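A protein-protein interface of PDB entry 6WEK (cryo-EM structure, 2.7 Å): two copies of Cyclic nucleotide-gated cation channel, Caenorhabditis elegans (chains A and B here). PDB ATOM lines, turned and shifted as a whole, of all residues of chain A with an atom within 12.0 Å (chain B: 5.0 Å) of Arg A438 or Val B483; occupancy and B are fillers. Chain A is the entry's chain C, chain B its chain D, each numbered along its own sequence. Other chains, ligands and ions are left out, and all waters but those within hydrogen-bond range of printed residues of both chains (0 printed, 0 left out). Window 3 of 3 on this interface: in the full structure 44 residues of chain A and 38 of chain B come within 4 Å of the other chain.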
ATOM      1  N   ASP A 429      21.671 -35.984 -13.834  1.00  0.00           N
ATOM      2  CA  ASP A 429      21.334 -35.228 -15.035  1.00  0.00           C
ATOM      3  C   ASP A 429      20.104 -34.368 -14.816  1.00  0.00           C
ATOM      4  O   ASP A 429      20.060 -33.215 -15.256  1.00  0.00           O
ATOM      5  CB  ASP A 429      21.097 -36.170 -16.210  1.00  0.00           C
ATOM      6  CG  ASP A 429      22.323 -36.953 -16.589  1.00  0.00           C
ATOM      7  OD1 ASP A 429      23.349 -36.833 -15.890  1.00  0.00           O
ATOM      8  OD2 ASP A 429      22.260 -37.692 -17.590  1.00  0.00           O
ATOM      9  N   GLY A 430      19.084 -34.912 -14.152  1.00  0.00           N
ATOM     10  CA  GLY A 430      17.903 -34.117 -13.876  1.00  0.00           C
ATOM     11  C   GLY A 430      18.217 -32.891 -13.047  1.00  0.00           C
ATOM     12  O   GLY A 430      17.728 -31.795 -13.330  1.00  0.00           O
ATOM     13  N   ILE A 431      19.057 -33.049 -12.026  1.00  0.00           N
ATOM     14  CA  ILE A 431      19.389 -31.908 -11.178  1.00  0.00           C
ATOM     15  C   ILE A 431      20.218 -30.888 -11.940  1.00  0.00           C
ATOM     16  O   ILE A 431      19.983 -29.681 -11.832  1.00  0.00           O
ATOM     17  CB  ILE A 431      20.104 -32.371  -9.904  1.00  0.00           C
ATOM     18  CG1 ILE A 431      19.140 -33.155  -9.031  1.00  0.00           C
ATOM     19  CG2 ILE A 431      20.637 -31.183  -9.148  1.00  0.00           C
ATOM     20  CD1 ILE A 431      19.563 -33.214  -7.621  1.00  0.00           C
ATOM     21  N   LYS A 432      21.210 -31.340 -12.704  1.00  0.00           N
ATOM     22  CA  LYS A 432      22.014 -30.397 -13.473  1.00  0.00           C
ATOM     23  C   LYS A 432      21.153 -29.621 -14.457  1.00  0.00           C
ATOM     24  O   LYS A 432      21.323 -28.406 -14.626  1.00  0.00           O
ATOM     25  CB  LYS A 432      23.131 -31.135 -14.204  1.00  0.00           C
ATOM     26  CG  LYS A 432      24.267 -31.562 -13.308  1.00  0.00           C
ATOM     27  CD  LYS A 432      25.501 -31.922 -14.105  1.00  0.00           C
ATOM     28  CE  LYS A 432      25.412 -33.321 -14.646  1.00  0.00           C
ATOM     29  NZ  LYS A 432      26.608 -33.656 -15.440  1.00  0.00           N
ATOM     30  N   GLN A 433      20.211 -30.303 -15.103  1.00  0.00           N
ATOM     31  CA  GLN A 433      19.343 -29.639 -16.061  1.00  0.00           C
ATOM     32  C   GLN A 433      18.422 -28.644 -15.376  1.00  0.00           C
ATOM     33  O   GLN A 433      18.172 -27.560 -15.911  1.00  0.00           O
ATOM     34  CB  GLN A 433      18.541 -30.683 -16.825  1.00  0.00           C
ATOM     35  CG  GLN A 433      17.870 -30.171 -18.062  1.00  0.00           C
ATOM     36  CD  GLN A 433      17.350 -31.301 -18.914  1.00  0.00           C
ATOM     37  OE1 GLN A 433      16.234 -31.245 -19.426  1.00  0.00           O
ATOM     38  NE2 GLN A 433      18.157 -32.342 -19.068  1.00  0.00           N
ATOM     39  N   TYR A 434      17.903 -28.986 -14.197  1.00  0.00           N
ATOM     40  CA  TYR A 434      17.128 -28.011 -13.441  1.00  0.00           C
ATOM     41  C   TYR A 434      17.958 -26.780 -13.123  1.00  0.00           C
ATOM     42  O   TYR A 434      17.512 -25.649 -13.332  1.00  0.00           O
ATOM     43  CB  TYR A 434      16.602 -28.629 -12.148  1.00  0.00           C
ATOM     44  CG  TYR A 434      15.956 -27.629 -11.217  1.00  0.00           C
ATOM     45  CD1 TYR A 434      16.698 -26.957 -10.261  1.00  0.00           C
ATOM     46  CD2 TYR A 434      14.604 -27.359 -11.294  1.00  0.00           C
ATOM     47  CE1 TYR A 434      16.113 -26.041  -9.419  1.00  0.00           C
ATOM     48  CE2 TYR A 434      14.012 -26.449 -10.453  1.00  0.00           C
ATOM     49  CZ  TYR A 434      14.769 -25.794  -9.519  1.00  0.00           C
ATOM     50  OH  TYR A 434      14.176 -24.887  -8.678  1.00  0.00           O
ATOM     51  N   MET A 435      19.172 -26.978 -12.616  1.00  0.00           N
ATOM     52  CA  MET A 435      19.953 -25.849 -12.127  1.00  0.00           C
ATOM     53  C   MET A 435      20.452 -24.967 -13.257  1.00  0.00           C
ATOM     54  O   MET A 435      20.696 -23.777 -13.038  1.00  0.00           O
ATOM     55  CB  MET A 435      21.131 -26.338 -11.295  1.00  0.00           C
ATOM     56  CG  MET A 435      20.740 -27.190 -10.120  1.00  0.00           C
ATOM     57  SD  MET A 435      22.166 -27.595  -9.122  1.00  0.00           S
ATOM     58  CE  MET A 435      22.378 -26.036  -8.291  1.00  0.00           C
ATOM     59  N   GLU A 436      20.637 -25.515 -14.457  1.00  0.00           N
ATOM     60  CA  GLU A 436      21.099 -24.663 -15.550  1.00  0.00           C
ATOM     61  C   GLU A 436      19.968 -23.801 -16.094  1.00  0.00           C
ATOM     62  O   GLU A 436      20.200 -22.667 -16.526  1.00  0.00           O
ATOM     63  CB  GLU A 436      21.723 -25.501 -16.662  1.00  0.00           C
ATOM     64  CG  GLU A 436      20.738 -26.260 -17.515  1.00  0.00           C
ATOM     65  CD  GLU A 436      21.378 -26.847 -18.752  1.00  0.00           C
ATOM     66  OE1 GLU A 436      22.594 -26.650 -18.944  1.00  0.00           O
ATOM     67  OE2 GLU A 436      20.662 -27.506 -19.533  1.00  0.00           O
ATOM     68  N   LEU A 437      18.738 -24.315 -16.075  1.00  0.00           N
ATOM     69  CA  LEU A 437      17.594 -23.529 -16.520  1.00  0.00           C
ATOM     70  C   LEU A 437      17.353 -22.346 -15.598  1.00  0.00           C
ATOM     71  O   LEU A 437      17.244 -21.201 -16.048  1.00  0.00           O
ATOM     72  CB  LEU A 437      16.348 -24.404 -16.579  1.00  0.00           C
ATOM     73  CG  LEU A 437      15.982 -25.044 -17.913  1.00  0.00           C
ATOM     74  CD1 LEU A 437      17.142 -25.837 -18.479  1.00  0.00           C
ATOM     75  CD2 LEU A 437      14.763 -25.927 -17.734  1.00  0.00           C
ATOM     76  N   ARG A 438      17.271 -22.605 -14.298  1.00  0.00           N
ATOM     77  CA  ARG A 438      16.945 -21.581 -13.317  1.00  0.00           C
ATOM     78  C   ARG A 438      18.101 -20.651 -13.019  1.00  0.00           C
ATOM     79  O   ARG A 438      17.939 -19.751 -12.189  1.00  0.00           O
ATOM     80  CB  ARG A 438      16.470 -22.234 -12.027  1.00  0.00           C
ATOM     81  CG  ARG A 438      14.989 -22.497 -11.985  1.00  0.00           C
ATOM     82  CD  ARG A 438      14.573 -23.584 -12.937  1.00  0.00           C
ATOM     83  NE  ARG A 438      13.132 -23.795 -12.884  1.00  0.00           N
ATOM     84  CZ  ARG A 438      12.495 -24.773 -13.515  1.00  0.00           C
ATOM     85  NH1 ARG A 438      13.167 -25.642 -14.255  1.00  0.00           N
ATOM     86  NH2 ARG A 438      11.180 -24.884 -13.403  1.00  0.00           N
ATOM     87  N   LYS A 439      19.247 -20.843 -13.662  1.00  0.00           N
ATOM     88  CA  LYS A 439      20.411 -19.978 -13.504  1.00  0.00           C
ATOM     89  C   LYS A 439      20.795 -19.832 -12.032  1.00  0.00           C
ATOM     90  O   LYS A 439      20.902 -18.733 -11.488  1.00  0.00           O
ATOM     91  CB  LYS A 439      20.164 -18.617 -14.153  1.00  0.00           C
ATOM     92  CG  LYS A 439      19.905 -18.694 -15.640  1.00  0.00           C
ATOM     93  CD  LYS A 439      19.547 -17.334 -16.204  1.00  0.00           C
ATOM     94  CE  LYS A 439      19.247 -17.414 -17.689  1.00  0.00           C
ATOM     95  NZ  LYS A 439      18.962 -16.072 -18.266  1.00  0.00           N
ATOM     96  N   VAL A 440      20.990 -20.972 -11.392  1.00  0.00           N
ATOM     97  CA  VAL A 440      21.534 -21.001 -10.043  1.00  0.00           C
ATOM     98  C   VAL A 440      23.014 -20.654 -10.115  1.00  0.00           C
ATOM     99  O   VAL A 440      23.700 -20.987 -11.086  1.00  0.00           O
ATOM    100  CB  VAL A 440      21.296 -22.382  -9.399  1.00  0.00           C
ATOM    101  CG1 VAL A 440      21.814 -22.419  -7.994  1.00  0.00           C
ATOM    102  CG2 VAL A 440      19.826 -22.712  -9.405  1.00  0.00           C
ATOM    103  N   SER A 441      23.513 -19.967  -9.089  1.00  0.00           N
ATOM    104  CA  SER A 441      24.897 -19.529  -9.093  1.00  0.00           C
ATOM    105  C   SER A 441      25.832 -20.720  -9.233  1.00  0.00           C
ATOM    106  O   SER A 441      25.484 -21.856  -8.916  1.00  0.00           O
ATOM    107  CB  SER A 441      25.226 -18.767  -7.815  1.00  0.00           C
ATOM    108  OG  SER A 441      25.123 -19.613  -6.691  1.00  0.00           O
ATOM    109  N   LYS A 442      27.041 -20.449  -9.722  1.00  0.00           N
ATOM    110  CA  LYS A 442      27.979 -21.531  -9.979  1.00  0.00           C
ATOM    111  C   LYS A 442      28.560 -22.098  -8.695  1.00  0.00           C
ATOM    112  O   LYS A 442      28.907 -23.280  -8.647  1.00  0.00           O
ATOM    113  CB  LYS A 442      29.098 -21.053 -10.898  1.00  0.00           C
ATOM    114  CG  LYS A 442      29.950 -22.178 -11.437  1.00  0.00           C
ATOM    115  CD  LYS A 442      30.986 -21.674 -12.418  1.00  0.00           C
ATOM    116  CE  LYS A 442      31.874 -22.809 -12.889  1.00  0.00           C
ATOM    117  NZ  LYS A 442      31.074 -23.948 -13.417  1.00  0.00           N
ATOM    118  N   GLN A 443      28.666 -21.284  -7.649  1.00  0.00           N
ATOM    119  CA  GLN A 443      29.153 -21.787  -6.370  1.00  0.00           C
ATOM    120  C   GLN A 443      28.224 -22.858  -5.813  1.00  0.00           C
ATOM    121  O   GLN A 443      28.663 -23.952  -5.442  1.00  0.00           O
ATOM    122  CB  GLN A 443      29.300 -20.631  -5.390  1.00  0.00           C
ATOM    123  CG  GLN A 443      29.758 -21.036  -4.014  1.00  0.00           C
ATOM    124  CD  GLN A 443      30.001 -19.840  -3.126  1.00  0.00           C
ATOM    125  OE1 GLN A 443      30.225 -19.979  -1.926  1.00  0.00           O
ATOM    126  NE2 GLN A 443      29.958 -18.651  -3.713  1.00  0.00           N
ATOM    127  N   LEU A 444      26.925 -22.561  -5.759  1.00  0.00           N
ATOM    128  CA  LEU A 444      25.962 -23.544  -5.282  1.00  0.00           C
ATOM    129  C   LEU A 444      25.888 -24.748  -6.206  1.00  0.00           C
ATOM    130  O   LEU A 444      25.695 -25.878  -5.744  1.00  0.00           O
ATOM    131  CB  LEU A 444      24.592 -22.889  -5.142  1.00  0.00           C
ATOM    132  CG  LEU A 444      23.440 -23.762  -4.666  1.00  0.00           C
ATOM    133  CD1 LEU A 444      23.790 -24.451  -3.370  1.00  0.00           C
ATOM    134  CD2 LEU A 444      22.229 -22.901  -4.484  1.00  0.00           C
ATOM    135  N   GLU A 445      26.059 -24.535  -7.505  1.00  0.00           N
ATOM    136  CA  GLU A 445      26.006 -25.647  -8.443  1.00  0.00           C
ATOM    137  C   GLU A 445      27.170 -26.606  -8.232  1.00  0.00           C
ATOM    138  O   GLU A 445      26.985 -27.828  -8.224  1.00  0.00           O
ATOM    139  CB  GLU A 445      25.989 -25.115  -9.869  1.00  0.00           C
ATOM    140  CG  GLU A 445      26.097 -26.185 -10.918  1.00  0.00           C
ATOM    141  CD  GLU A 445      25.701 -25.685 -12.282  1.00  0.00           C
ATOM    142  OE1 GLU A 445      25.229 -24.534 -12.378  1.00  0.00           O
ATOM    143  OE2 GLU A 445      25.856 -26.442 -13.261  1.00  0.00           O
ATOM    144  N   ARG A 447      28.778 -26.913  -5.462  1.00  0.00           N
ATOM    145  CA  ARG A 447      28.565 -27.556  -4.171  1.00  0.00           C
ATOM    146  C   ARG A 447      27.647 -28.763  -4.301  1.00  0.00           C
ATOM    147  O   ARG A 447      27.925 -29.829  -3.740  1.00  0.00           O
ATOM    148  CB  ARG A 447      27.997 -26.566  -3.164  1.00  0.00           C
ATOM    149  CG  ARG A 447      27.547 -27.235  -1.888  1.00  0.00           C
ATOM    150  CD  ARG A 447      27.792 -26.379  -0.662  1.00  0.00           C
ATOM    151  NE  ARG A 447      26.812 -25.313  -0.516  1.00  0.00           N
ATOM    152  CZ  ARG A 447      27.008 -24.063  -0.917  1.00  0.00           C
ATOM    153  NH1 ARG A 447      28.149 -23.724  -1.494  1.00  0.00           N
ATOM    154  NH2 ARG A 447      26.063 -23.154  -0.741  1.00  0.00           N
ATOM    155  N   VAL A 448      26.560 -28.624  -5.059  1.00  0.00           N
ATOM    156  CA  VAL A 448      25.654 -29.750  -5.266  1.00  0.00           C
ATOM    157  C   VAL A 448      26.352 -30.877  -6.020  1.00  0.00           C
ATOM    158  O   VAL A 448      26.204 -32.061  -5.684  1.00  0.00           O
ATOM    159  CB  VAL A 448      24.391 -29.277  -6.001  1.00  0.00           C
ATOM    160  CG1 VAL A 448      23.554 -30.454  -6.414  1.00  0.00           C
ATOM    161  CG2 VAL A 448      23.592 -28.349  -5.122  1.00  0.00           C
ATOM    162  N   LYS B 459       8.515 -24.712 -19.196  1.00  0.00           N
ATOM    163  CA  LYS B 459       9.312 -25.764 -18.561  1.00  0.00           C
ATOM    164  C   LYS B 459       9.073 -25.847 -17.054  1.00  0.00           C
ATOM    165  O   LYS B 459      10.005 -26.013 -16.264  1.00  0.00           O
ATOM    166  CB  LYS B 459      10.795 -25.570 -18.865  1.00  0.00           C
ATOM    167  CG  LYS B 459      11.122 -25.652 -20.341  1.00  0.00           C
ATOM    168  CD  LYS B 459      10.626 -26.953 -20.936  1.00  0.00           C
ATOM    169  CE  LYS B 459      11.070 -27.085 -22.374  1.00  0.00           C
ATOM    170  NZ  LYS B 459      10.750 -25.859 -23.148  1.00  0.00           N
ATOM    171  N   GLN B 460       7.811 -25.732 -16.652  1.00  0.00           N
ATOM    172  CA  GLN B 460       7.408 -25.924 -15.266  1.00  0.00           C
ATOM    173  C   GLN B 460       6.761 -27.282 -15.032  1.00  0.00           C
ATOM    174  O   GLN B 460       6.163 -27.495 -13.972  1.00  0.00           O
ATOM    175  CB  GLN B 460       6.440 -24.821 -14.841  1.00  0.00           C
ATOM    176  CG  GLN B 460       6.975 -23.417 -14.995  1.00  0.00           C
ATOM    177  CD  GLN B 460       5.933 -22.467 -15.528  1.00  0.00           C
ATOM    178  OE1 GLN B 460       5.206 -22.792 -16.461  1.00  0.00           O
ATOM    179  NE2 GLN B 460       5.848 -21.285 -14.935  1.00  0.00           N
ATOM    180  N   SER B 463       9.749 -30.249 -13.157  1.00  0.00           N
ATOM    181  CA  SER B 463      11.160 -30.086 -12.828  1.00  0.00           C
ATOM    182  C   SER B 463      11.286 -29.404 -11.476  1.00  0.00           C
ATOM    183  O   SER B 463      11.859 -28.320 -11.367  1.00  0.00           O
ATOM    184  CB  SER B 463      11.871 -29.290 -13.916  1.00  0.00           C
ATOM    185  OG  SER B 463      11.321 -27.988 -14.029  1.00  0.00           O
ATOM    186  N   ILE B 479      18.992 -23.758  -2.550  1.00  0.00           N
ATOM    187  CA  ILE B 479      18.711 -23.609  -3.975  1.00  0.00           C
ATOM    188  C   ILE B 479      17.430 -22.820  -4.188  1.00  0.00           C
ATOM    189  O   ILE B 479      17.397 -21.868  -4.974  1.00  0.00           O
ATOM    190  CB  ILE B 479      18.626 -24.986  -4.654  1.00  0.00           C
ATOM    191  CG1 ILE B 479      19.975 -25.690  -4.621  1.00  0.00           C
ATOM    192  CG2 ILE B 479      18.143 -24.840  -6.073  1.00  0.00           C
ATOM    193  CD1 ILE B 479      19.947 -27.040  -5.262  1.00  0.00           C
ATOM    194  N   ALA B 480      16.354 -23.196  -3.492  1.00  0.00           N
ATOM    195  CA  ALA B 480      15.076 -22.523  -3.682  1.00  0.00           C
ATOM    196  C   ALA B 480      15.143 -21.073  -3.242  1.00  0.00           C
ATOM    197  O   ALA B 480      14.552 -20.197  -3.881  1.00  0.00           O
ATOM    198  CB  ALA B 480      13.981 -23.258  -2.918  1.00  0.00           C
ATOM    199  N   MET B 481      15.852 -20.791  -2.153  1.00  0.00           N
ATOM    200  CA  MET B 481      15.961 -19.415  -1.697  1.00  0.00           C
ATOM    201  C   MET B 481      16.795 -18.590  -2.660  1.00  0.00           C
ATOM    202  O   MET B 481      16.658 -17.365  -2.712  1.00  0.00           O
ATOM    203  CB  MET B 481      16.553 -19.377  -0.294  1.00  0.00           C
ATOM    204  CG  MET B 481      15.663 -18.697   0.714  1.00  0.00           C
ATOM    205  SD  MET B 481      16.320 -18.775   2.385  1.00  0.00           S
ATOM    206  CE  MET B 481      16.185 -20.524   2.704  1.00  0.00           C
ATOM    207  N   GLN B 482      17.672 -19.237  -3.422  1.00  0.00           N
ATOM    208  CA  GLN B 482      18.421 -18.497  -4.429  1.00  0.00           C
ATOM    209  C   GLN B 482      17.614 -18.308  -5.707  1.00  0.00           C
ATOM    210  O   GLN B 482      17.644 -17.232  -6.308  1.00  0.00           O
ATOM    211  CB  GLN B 482      19.735 -19.201  -4.731  1.00  0.00           C
ATOM    212  CG  GLN B 482      20.485 -18.566  -5.865  1.00  0.00           C
ATOM    213  CD  GLN B 482      21.849 -19.155  -6.045  1.00  0.00           C
ATOM    214  OE1 GLN B 482      22.348 -19.249  -7.162  1.00  0.00           O
ATOM    215  NE2 GLN B 482      22.468 -19.557  -4.945  1.00  0.00           N
ATOM    216  N   VAL B 483      16.889 -19.341  -6.141  1.00  0.00           N
ATOM    217  CA  VAL B 483      16.154 -19.262  -7.400  1.00  0.00           C
ATOM    218  C   VAL B 483      15.060 -18.207  -7.324  1.00  0.00           C
ATOM    219  O   VAL B 483      14.899 -17.393  -8.239  1.00  0.00           O
ATOM    220  CB  VAL B 483      15.575 -20.636  -7.765  1.00  0.00           C
ATOM    221  CG1 VAL B 483      14.614 -20.500  -8.904  1.00  0.00           C
ATOM    222  CG2 VAL B 483      16.678 -21.585  -8.130  1.00  0.00           C
ATOM    223  N   HIS B 484      14.291 -18.204  -6.240  1.00  0.00           N
ATOM    224  CA  HIS B 484      13.178 -17.283  -6.058  1.00  0.00           C
ATOM    225  C   HIS B 484      13.578 -16.075  -5.226  1.00  0.00           C
ATOM    226  O   HIS B 484      12.763 -15.534  -4.482  1.00  0.00           O
ATOM    227  CB  HIS B 484      11.998 -17.993  -5.404  1.00  0.00           C
ATOM    228  CG  HIS B 484      11.645 -19.295  -6.046  1.00  0.00           C
ATOM    229  ND1 HIS B 484      11.270 -19.397  -7.366  1.00  0.00           N
ATOM    230  CD2 HIS B 484      11.600 -20.549  -5.544  1.00  0.00           C
ATOM    231  CE1 HIS B 484      11.015 -20.659  -7.653  1.00  0.00           C
ATOM    232  NE2 HIS B 484      11.207 -21.379  -6.563  1.00  0.00           N
ATOM    233  N   PHE B 485      14.834 -15.646  -5.335  1.00  0.00           N
ATOM    234  CA  PHE B 485      15.320 -14.575  -4.476  1.00  0.00           C
ATOM    235  C   PHE B 485      14.646 -13.251  -4.796  1.00  0.00           C
ATOM    236  O   PHE B 485      14.203 -12.537  -3.890  1.00  0.00           O
ATOM    237  CB  PHE B 485      16.835 -14.446  -4.608  1.00  0.00           C
ATOM    238  CG  PHE B 485      17.392 -13.220  -3.955  1.00  0.00           C
ATOM    239  CD1 PHE B 485      17.460 -13.124  -2.579  1.00  0.00           C
ATOM    240  CD2 PHE B 485      17.851 -12.166  -4.718  1.00  0.00           C
ATOM    241  CE1 PHE B 485      17.965 -12.000  -1.980  1.00  0.00           C
ATOM    242  CE2 PHE B 485      18.357 -11.040  -4.121  1.00  0.00           C
ATOM    243  CZ  PHE B 485      18.415 -10.958  -2.751  1.00  0.00           C
ATOM    244  N   GLU B 486      14.561 -12.900  -6.075  1.00  0.00           N
ATOM    245  CA  GLU B 486      13.973 -11.617  -6.440  1.00  0.00           C
ATOM    246  C   GLU B 486      12.474 -11.604  -6.176  1.00  0.00           C
ATOM    247  O   GLU B 486      11.895 -10.544  -5.924  1.00  0.00           O
ATOM    248  CB  GLU B 486      14.271 -11.292  -7.905  1.00  0.00           C
ATOM    249  CG  GLU B 486      13.504 -12.120  -8.920  1.00  0.00           C
ATOM    250  CD  GLU B 486      13.989 -13.553  -9.008  1.00  0.00           C
ATOM    251  OE1 GLU B 486      15.122 -13.829  -8.564  1.00  0.00           O
ATOM    252  OE2 GLU B 486      13.233 -14.403  -9.523  1.00  0.00           O
ATOM    253  N   LYS B 534       4.059 -15.388  -7.916  1.00  0.00           N
ATOM    254  CA  LYS B 534       5.372 -15.576  -8.511  1.00  0.00           C
ATOM    255  C   LYS B 534       5.488 -14.857  -9.844  1.00  0.00           C
ATOM    256  O   LYS B 534       6.466 -14.145 -10.082  1.00  0.00           O
ATOM    257  CB  LYS B 534       5.649 -17.070  -8.687  1.00  0.00           C
ATOM    258  CG  LYS B 534       6.904 -17.406  -9.458  1.00  0.00           C
ATOM    259  CD  LYS B 534       8.137 -16.861  -8.776  1.00  0.00           C
ATOM    260  CE  LYS B 534       9.394 -17.240  -9.528  1.00  0.00           C
ATOM    261  NZ  LYS B 534      10.579 -16.533  -8.983  1.00  0.00           N
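O of Lys B459 is in hydrogen-bond range of NH2 of Arg A438 (3.3 Å).
The guanidinium group (NH1) of Arg A438 lies within hydrogen-bond range of the side-chain hydroxyl (OG) of Ser B463 (3.0 Å).
OE1 of Gln B482 lies within hydrogen-bond range of OG of Ser A441, at 2.8 Å.
The backbone carbonyl oxygen (O) of Met A435 is in hydrogen-bond range of the backbone NH (N) of Val A440, at 3.3 Å.
The backbone carbonyl oxygen (O) of Lys B459 lies within hydrogen-bond range of the side-chain hydroxyl (OG) of Ser B463 (3.3 Å).
Tyr A434 touches Ser B463.
CG of Arg A438 touches CG1 of Val B483 (3.7 Å).
Gln B482 touches Val A440.
Val A440 touches Val B483.
CD2 of Leu A444 touches CG1 of Ile B479, at 3.6 Å.
CD2 of Leu A444 touches NE2 of Gln B482, at 3.4 Å.
Val A448 touches Ile B479 (CG2 to CD1, 3.9 Å).
Printed residues of chain B within 4 Å of Arg A438: Lys B459, Ser B463 and Val B483.
No residue of chain A comes within 4 Å of Gln B460.
Ser B463 touches just these residues of chain A: Tyr A434 and Arg A438.
Of chain A, only Val A440, Ser A441 and Leu A444 come within 4 Å of Gln B482.
Printed residues of chain A within 4 Å of Ile B479: Leu A444 (3.6 Å) and Val A448 (3.9 Å).
Printed residues of chain B within 4 Å of Tyr A434: Ser B463 (2.9 Å).
Of the printed residues of chain B, Val A448 touches Ile B479.
Of the printed residues of chain B, Val A440 touches Gln B482 (3.3 Å) and Val B483 (3.6 Å).
Printed residues of chain B within 4 Å of Leu A444: Ile B479 and Gln B482.
The nearest residue of chain A that does not touch Val B483 is Tyr A434 (4.2 Å).
The nearest printed residue of chain B that does not touch Val A440 is Ile B479 (4.3 Å).
Of the 12 printed residues of chain B, 5 touch a printed residue of chain A.
Among the printed residues, 10 pairs touch across the chains.
Among the printed residues, no Asp or Glu carboxylate lies within 4 Å of a Lys or Arg side-chain nitrogen of the other chain.
No position is printed for both chains.
Of the 10 pairs that touch across the chains among the printed residues, none has its exchanged pair printed and touching as well.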
